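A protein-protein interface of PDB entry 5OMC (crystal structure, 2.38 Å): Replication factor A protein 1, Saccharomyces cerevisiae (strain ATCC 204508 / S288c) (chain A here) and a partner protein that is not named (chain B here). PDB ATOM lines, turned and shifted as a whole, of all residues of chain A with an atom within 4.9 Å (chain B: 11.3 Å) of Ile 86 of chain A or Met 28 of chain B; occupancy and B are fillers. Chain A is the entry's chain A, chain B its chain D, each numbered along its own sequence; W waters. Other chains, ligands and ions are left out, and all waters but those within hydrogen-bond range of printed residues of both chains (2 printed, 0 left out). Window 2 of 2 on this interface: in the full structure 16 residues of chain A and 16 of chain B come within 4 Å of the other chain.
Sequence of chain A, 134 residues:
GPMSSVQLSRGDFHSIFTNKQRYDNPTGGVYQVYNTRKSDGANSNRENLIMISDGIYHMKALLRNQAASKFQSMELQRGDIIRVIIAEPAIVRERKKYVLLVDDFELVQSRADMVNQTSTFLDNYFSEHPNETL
Water W2 lies within hydrogen-bond range of the side-chain carboxylate of Glu 88 of chain A (2.6 Å), the guanidinium group of Arg 22 of chain B (2.8 Å) and the backbone carbonyl oxygen of Pro 23 of chain B (2.9 Å). Water W1 lies within hydrogen-bond range of OE2 of Glu 88 of chain A (2.9 Å), OD2 of Asp 103 of chain A (2.9 Å) and N of Ser 26 of chain B (3.2 Å).
Hydrophobic or aromatic side chains of chain B within 4 Å of the printed part of chain A: Pro 24, Met 25, Met 28, Ala 29 and Val 30. Of the 11 printed residues of chain A, 5 touch a printed residue of chain B. Hydrophobic or aromatic side chains of chain A within 4 Å of the printed part of chain B: Ile 86 and Leu 101. Along chain A the printed residues that touch a printed residue of chain B span positions 66 to 103. Among the printed residues, Asp or Glu carboxylates within 4 Å of a Lys or Arg side-chain nitrogen of the other chain: Glu 88 of chain A with Arg 22 of chain B (3.0 Å).
NH2 of Arg 22 of chain B is in salt-bridge range of OE1 of Glu 88 of chain A. OE2 of Glu 88 of chain A lies within hydrogen-bond range of N of Met 25 of chain B (2.8 Å). The side-chain amide nitrogen (NE2) of Gln 66 of chain A sits at hydrogen-bond distance from the backbone carbonyl oxygen (O) of Met 28 of chain B, 3.1 Å away. N of Val 30 of chain B is in hydrogen-bond range of OE1 of Gln 66 of chain A (3.0 Å).
OD2 of Asp 104 of chain A is in hydrogen-bond range of NE2 of Gln 66 of chain A, at 3.4 Å. The side-chain amide oxygen (OE1) of Gln 66 of chain A sits close to the backbone carbonyl oxygen (O) of Asp 103 of chain A. The backbone carbonyl oxygen (O) of Asp 104 of chain A is in hydrogen-bond range of the backbone NH (N) of Ile 86 of chain A. N of Leu 101 of chain A lies within hydrogen-bond range of O of Glu 88 of chain A (2.8 Å). The backbone NH of Met 28 of chain B lies within hydrogen-bond range of the side-chain hydroxyl of Ser 26 of chain B (3.1 Å). The backbone NH of Asp 103 of chain A lies within hydrogen-bond range of the backbone carbonyl oxygen of Ile 86 of chain A (2.8 Å).
Ile 86 of chain A touches two residues of chain B. No residue of chain B comes within 4 Å of Ile 85 of chain A. No residue of chain B comes within 4 Å of Ala 87 of chain A. Asp 103 of chain A touches just one residue of chain B: Ala 29 (3.8 Å). No residue of chain B comes within 4 Å of Asp 104 of chain A. Of the printed residues of chain A, Ser 26 of chain B touches Ile 86. Printed residues of chain A within 4 Å of Arg 22 of chain B: Glu 88 (3.0 Å) and Leu 101 (3.3 Å). Of the printed residues of chain B, Leu 101 of chain A touches Arg 22 (3.3 Å). Printed residues of chain A within 4 Å of Met 25 of chain B: Glu 88. Printed residues of chain A within 4 Å of Val 30 of chain B: Gln 66. Pro 31 of chain B touches none of the printed residues of chain A. The nearest printed residue of chain A that does not touch Met 28 of chain B is Asp 104 of chain A (5.6 Å).
Among the printed residues, merely in contact across the chains: Gln 66 of chain A with Ala 29 of chain B (3.4 Å), Ile 86 of chain A with Ser 26 of chain B (3.6 Å), Ile 86 of chain A with Met 28 of chain B (3.8 Å), Glu 88 of chain A with Pro 24 of chain B (3.3 Å), Leu 101 of chain A with Arg 22 of chain B (3.3 Å) and Asp 103 of chain A with Ala 29 of chain B (3.8 Å).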
ATOM      1  N   THR A  27     -10.740 -16.474  15.681  1.00  0.00           N
ATOM      2  CA  THR A  27     -11.207 -17.238  14.523  1.00  0.00           C
ATOM      3  C   THR A  27     -11.980 -18.476  14.967  1.00  0.00           C
ATOM      4  O   THR A  27     -11.893 -18.863  16.139  1.00  0.00           O
ATOM      5  CB  THR A  27     -10.018 -17.591  13.619  1.00  0.00           C
ATOM      6  OG1 THR A  27      -9.083 -18.359  14.383  1.00  0.00           O
ATOM      7  CG2 THR A  27      -9.339 -16.356  13.053  1.00  0.00           C
ATOM      8  N   GLN A  66     -10.231 -10.550   1.296  1.00  0.00           N
ATOM      9  CA  GLN A  66     -11.071 -11.604   0.679  1.00  0.00           C
ATOM     10  C   GLN A  66     -12.545 -11.566   1.148  1.00  0.00           C
ATOM     11  O   GLN A  66     -13.438 -11.816   0.345  1.00  0.00           O
ATOM     12  CB  GLN A  66     -10.544 -13.032   0.993  1.00  0.00           C
ATOM     13  CG  GLN A  66      -9.049 -13.259   0.924  1.00  0.00           C
ATOM     14  CD  GLN A  66      -8.390 -13.039   2.244  1.00  0.00           C
ATOM     15  OE1 GLN A  66      -8.147 -11.922   2.626  1.00  0.00           O
ATOM     16  NE2 GLN A  66      -8.009 -14.082   2.937  1.00  0.00           N
ATOM     17  N   VAL A  84     -16.000 -17.296  10.801  1.00  0.00           N
ATOM     18  CA  VAL A  84     -14.849 -16.424  10.660  1.00  0.00           C
ATOM     19  C   VAL A  84     -13.569 -17.267  10.654  1.00  0.00           C
ATOM     20  O   VAL A  84     -13.375 -18.098  11.553  1.00  0.00           O
ATOM     21  CB  VAL A  84     -14.873 -15.315  11.728  1.00  0.00           C
ATOM     22  CG1 VAL A  84     -13.580 -14.528  11.708  1.00  0.00           C
ATOM     23  CG2 VAL A  84     -16.065 -14.392  11.509  1.00  0.00           C
ATOM     24  N   ILE A  85     -12.725 -17.070   9.603  1.00  0.00           N
ATOM     25  CA  ILE A  85     -11.472 -17.799   9.335  1.00  0.00           C
ATOM     26  C   ILE A  85     -10.255 -16.943   9.674  1.00  0.00           C
ATOM     27  O   ILE A  85      -9.280 -17.456  10.224  1.00  0.00           O
ATOM     28  CB  ILE A  85     -11.442 -18.309   7.861  1.00  0.00           C
ATOM     29  CG1 ILE A  85     -12.693 -19.185   7.495  1.00  0.00           C
ATOM     30  CG2 ILE A  85     -10.140 -19.007   7.513  1.00  0.00           C
ATOM     31  CD1 ILE A  85     -13.195 -20.209   8.487  1.00  0.00           C
ATOM     32  N   ILE A  86     -10.280 -15.654   9.286  1.00  0.00           N
ATOM     33  CA  ILE A  86      -9.207 -14.698   9.587  1.00  0.00           C
ATOM     34  C   ILE A  86      -9.834 -13.480  10.190  1.00  0.00           C
ATOM     35  O   ILE A  86     -10.685 -12.853   9.567  1.00  0.00           O
ATOM     36  CB  ILE A  86      -8.298 -14.344   8.376  1.00  0.00           C
ATOM     37  CG1 ILE A  86      -7.793 -15.600   7.620  1.00  0.00           C
ATOM     38  CG2 ILE A  86      -7.145 -13.450   8.832  1.00  0.00           C
ATOM     39  CD1 ILE A  86      -7.189 -15.301   6.370  1.00  0.00           C
ATOM     40  N   ALA A  87      -9.445 -13.144  11.408  1.00  0.00           N
ATOM     41  CA  ALA A  87      -9.998 -11.955  12.058  1.00  0.00           C
ATOM     42  C   ALA A  87      -9.007 -11.319  13.010  1.00  0.00           C
ATOM     43  O   ALA A  87      -8.071 -11.971  13.471  1.00  0.00           O
ATOM     44  CB  ALA A  87     -11.290 -12.303  12.804  1.00  0.00           C
ATOM     45  N   GLU A  88      -9.238 -10.036  13.312  1.00  0.00           N
ATOM     46  CA  GLU A  88      -8.481  -9.240  14.279  1.00  0.00           C
ATOM     47  C   GLU A  88      -9.447  -8.510  15.178  1.00  0.00           C
ATOM     48  O   GLU A  88     -10.376  -7.854  14.673  1.00  0.00           O
ATOM     49  CB  GLU A  88      -7.635  -8.181  13.589  1.00  0.00           C
ATOM     50  CG  GLU A  88      -6.426  -8.733  12.893  1.00  0.00           C
ATOM     51  CD  GLU A  88      -5.652  -7.676  12.149  1.00  0.00           C
ATOM     52  OE1 GLU A  88      -5.512  -6.551  12.679  1.00  0.00           O
ATOM     53  OE2 GLU A  88      -5.142  -7.992  11.053  1.00  0.00           O
ATOM     54  N   LEU A 101     -12.477  -7.171  12.900  1.00  0.00           N
ATOM     55  CA  LEU A 101     -11.999  -7.005  11.523  1.00  0.00           C
ATOM     56  C   LEU A 101     -11.943  -8.408  10.903  1.00  0.00           C
ATOM     57  O   LEU A 101     -11.141  -9.237  11.334  1.00  0.00           O
ATOM     58  CB  LEU A 101     -10.619  -6.300  11.469  1.00  0.00           C
ATOM     59  CG  LEU A 101     -10.430  -5.083  12.393  1.00  0.00           C
ATOM     60  CD1 LEU A 101      -8.979  -4.762  12.547  1.00  0.00           C
ATOM     61  CD2 LEU A 101     -11.223  -3.853  11.885  1.00  0.00           C
ATOM     62  N   VAL A 102     -12.847  -8.682   9.943  1.00  0.00           N
ATOM     63  CA  VAL A 102     -12.950 -10.003   9.299  1.00  0.00           C
ATOM     64  C   VAL A 102     -12.286  -9.971   7.928  1.00  0.00           C
ATOM     65  O   VAL A 102     -12.716  -9.214   7.065  1.00  0.00           O
ATOM     66  CB  VAL A 102     -14.418 -10.539   9.289  1.00  0.00           C
ATOM     67  CG1 VAL A 102     -14.521 -11.897   8.600  1.00  0.00           C
ATOM     68  CG2 VAL A 102     -14.967 -10.626  10.699  1.00  0.00           C
ATOM     69  N   ASP A 103     -11.191 -10.755   7.764  1.00  0.00           N
ATOM     70  CA  ASP A 103     -10.387 -10.827   6.535  1.00  0.00           C
ATOM     71  C   ASP A 103     -10.765 -12.013   5.687  1.00  0.00           C
ATOM     72  O   ASP A 103     -10.553 -11.987   4.480  1.00  0.00           O
ATOM     73  CB  ASP A 103      -8.876 -10.812   6.841  1.00  0.00           C
ATOM     74  CG  ASP A 103      -8.407  -9.505   7.477  1.00  0.00           C
ATOM     75  OD1 ASP A 103      -8.702  -8.443   6.922  1.00  0.00           O
ATOM     76  OD2 ASP A 103      -7.776  -9.554   8.564  1.00  0.00           O
ATOM     77  N   ASP A 104     -11.333 -13.052   6.308  1.00  0.00           N
ATOM     78  CA  ASP A 104     -11.809 -14.246   5.629  1.00  0.00           C
ATOM     79  C   ASP A 104     -12.831 -14.975   6.487  1.00  0.00           C
ATOM     80  O   ASP A 104     -12.722 -14.998   7.718  1.00  0.00           O
ATOM     81  CB  ASP A 104     -10.657 -15.174   5.255  1.00  0.00           C
ATOM     82  CG  ASP A 104     -10.933 -16.114   4.093  1.00  0.00           C
ATOM     83  OD1 ASP A 104     -12.093 -16.160   3.618  1.00  0.00           O
ATOM     84  OD2 ASP A 104      -9.985 -16.720   3.602  1.00  0.00           O
ATOM     85  N   ARG B  22      -5.591  -0.852   7.121  1.00  0.00           N
ATOM     86  CA  ARG B  22      -4.566  -1.106   8.128  1.00  0.00           C
ATOM     87  C   ARG B  22      -3.940  -2.436   7.779  1.00  0.00           C
ATOM     88  O   ARG B  22      -4.674  -3.387   7.502  1.00  0.00           O
ATOM     89  CB  ARG B  22      -5.150  -1.151   9.546  1.00  0.00           C
ATOM     90  CG  ARG B  22      -4.078  -1.006  10.623  1.00  0.00           C
ATOM     91  CD  ARG B  22      -4.632  -0.998  12.020  1.00  0.00           C
ATOM     92  NE  ARG B  22      -5.142  -2.310  12.395  1.00  0.00           N
ATOM     93  CZ  ARG B  22      -5.621  -2.611  13.595  1.00  0.00           C
ATOM     94  NH1 ARG B  22      -5.639  -1.697  14.562  1.00  0.00           N
ATOM     95  NH2 ARG B  22      -6.077  -3.832  13.846  1.00  0.00           N
ATOM     96  N   PRO B  23      -2.593  -2.506   7.674  1.00  0.00           N
ATOM     97  CA  PRO B  23      -1.967  -3.783   7.280  1.00  0.00           C
ATOM     98  C   PRO B  23      -2.413  -4.954   8.166  1.00  0.00           C
ATOM     99  O   PRO B  23      -2.419  -4.832   9.402  1.00  0.00           O
ATOM    100  CB  PRO B  23      -0.462  -3.511   7.379  1.00  0.00           C
ATOM    101  CG  PRO B  23      -0.337  -2.216   7.996  1.00  0.00           C
ATOM    102  CD  PRO B  23      -1.586  -1.452   7.904  1.00  0.00           C
ATOM    103  N   PRO B  24      -2.869  -6.069   7.568  1.00  0.00           N
ATOM    104  CA  PRO B  24      -3.314  -7.198   8.393  1.00  0.00           C
ATOM    105  C   PRO B  24      -2.178  -7.921   9.092  1.00  0.00           C
ATOM    106  O   PRO B  24      -1.059  -8.009   8.557  1.00  0.00           O
ATOM    107  CB  PRO B  24      -3.993  -8.144   7.382  1.00  0.00           C
ATOM    108  CG  PRO B  24      -4.055  -7.404   6.102  1.00  0.00           C
ATOM    109  CD  PRO B  24      -2.998  -6.371   6.132  1.00  0.00           C
ATOM    110  N   MET B  25      -2.485  -8.487  10.266  1.00  0.00           N
ATOM    111  CA  MET B  25      -1.566  -9.329  10.996  1.00  0.00           C
ATOM    112  C   MET B  25      -1.303 -10.617  10.221  1.00  0.00           C
ATOM    113  O   MET B  25      -0.179 -11.110  10.225  1.00  0.00           O
ATOM    114  CB  MET B  25      -2.168  -9.671  12.355  1.00  0.00           C
ATOM    115  CG  MET B  25      -1.920  -8.590  13.366  1.00  0.00           C
ATOM    116  SD  MET B  25      -0.193  -8.547  13.989  1.00  0.00           S
ATOM    117  CE  MET B  25       0.071 -10.258  14.572  1.00  0.00           C
ATOM    118  N   SER B  26      -2.331 -11.155   9.548  1.00  0.00           N
ATOM    119  CA  SER B  26      -2.191 -12.393   8.795  1.00  0.00           C
ATOM    120  C   SER B  26      -1.588 -12.165   7.461  1.00  0.00           C
ATOM    121  O   SER B  26      -1.943 -11.226   6.748  1.00  0.00           O
ATOM    122  CB  SER B  26      -3.526 -13.112   8.633  1.00  0.00           C
ATOM    123  OG  SER B  26      -3.351 -14.421   8.103  1.00  0.00           O
ATOM    124  N   GLN B  27      -0.675 -13.062   7.095  1.00  0.00           N
ATOM    125  CA  GLN B  27      -0.041 -13.042   5.780  1.00  0.00           C
ATOM    126  C   GLN B  27      -0.988 -13.668   4.758  1.00  0.00           C
ATOM    127  O   GLN B  27      -0.782 -13.506   3.557  1.00  0.00           O
ATOM    128  CB  GLN B  27       1.335 -13.738   5.815  1.00  0.00           C
ATOM    129  CG  GLN B  27       2.451 -12.802   6.284  1.00  0.00           C
ATOM    130  CD  GLN B  27       3.683 -13.526   6.780  1.00  0.00           C
ATOM    131  OE1 GLN B  27       3.999 -13.457   7.976  1.00  0.00           O
ATOM    132  NE2 GLN B  27       4.422 -14.219   5.891  1.00  0.00           N
ATOM    133  N   MET B  28      -2.042 -14.364   5.253  1.00  0.00           N
ATOM    134  CA  MET B  28      -3.074 -15.038   4.450  1.00  0.00           C
ATOM    135  C   MET B  28      -4.149 -14.067   3.971  1.00  0.00           C
ATOM    136  O   MET B  28      -4.882 -14.392   3.051  1.00  0.00           O
ATOM    137  CB  MET B  28      -3.717 -16.226   5.195  1.00  0.00           C
ATOM    138  CG  MET B  28      -2.741 -17.202   5.809  1.00  0.00           C
ATOM    139  SD  MET B  28      -1.829 -18.113   4.556  1.00  0.00           S
ATOM    140  CE  MET B  28      -0.251 -18.391   5.403  1.00  0.00           C
ATOM    141  N   ALA B  29      -4.241 -12.898   4.603  1.00  0.00           N
ATOM    142  CA  ALA B  29      -5.157 -11.810   4.271  1.00  0.00           C
ATOM    143  C   ALA B  29      -4.621 -11.055   3.040  1.00  0.00           C
ATOM    144  O   ALA B  29      -3.554 -10.432   3.084  1.00  0.00           O
ATOM    145  CB  ALA B  29      -5.310 -10.875   5.462  1.00  0.00           C
ATOM    146  N   VAL B  30      -5.339 -11.186   1.916  1.00  0.00           N
ATOM    147  CA  VAL B  30      -4.957 -10.587   0.642  1.00  0.00           C
ATOM    148  C   VAL B  30      -5.923  -9.504   0.201  1.00  0.00           C
ATOM    149  O   VAL B  30      -7.127  -9.747   0.102  1.00  0.00           O
ATOM    150  CB  VAL B  30      -4.704 -11.616  -0.490  1.00  0.00           C
ATOM    151  CG1 VAL B  30      -3.471 -12.453  -0.210  1.00  0.00           C
ATOM    152  CG2 VAL B  30      -5.905 -12.517  -0.737  1.00  0.00           C
ATOM    153  N   PRO B  31      -5.402  -8.305  -0.123  1.00  0.00           N
ATOM    154  CA  PRO B  31      -6.286  -7.257  -0.654  1.00  0.00           C
ATOM    155  C   PRO B  31      -6.795  -7.622  -2.045  1.00  0.00           C
ATOM    156  O   PRO B  31      -6.076  -8.217  -2.853  1.00  0.00           O
ATOM    157  CB  PRO B  31      -5.395  -6.012  -0.685  1.00  0.00           C
ATOM    158  CG  PRO B  31      -4.007  -6.535  -0.750  1.00  0.00           C
ATOM    159  CD  PRO B  31      -3.991  -7.867  -0.078  1.00  0.00           C
ATOM    160  N   ILE B  32      -8.058  -7.352  -2.287  1.00  0.00           N
ATOM    161  CA  ILE B  32      -8.659  -7.609  -3.575  1.00  0.00           C
ATOM    162  C   ILE B  32      -9.223  -6.283  -4.046  1.00  0.00           C
ATOM    163  O   ILE B  32     -10.076  -5.708  -3.364  1.00  0.00           O
ATOM    164  CB  ILE B  32      -9.771  -8.694  -3.562  1.00  0.00           C
ATOM    165  CG1 ILE B  32      -9.440  -9.911  -2.635  1.00  0.00           C
ATOM    166  CG2 ILE B  32     -10.093  -9.095  -5.010  1.00  0.00           C
ATOM    167  CD1 ILE B  32      -8.690 -11.049  -3.175  1.00  0.00           C
HETATM  168  O   HOH W   1      -5.450 -10.650   9.948  1.00  0.00           O
HETATM  169  O   HOH W   2      -4.896  -4.688  10.965  1.00  0.00           O
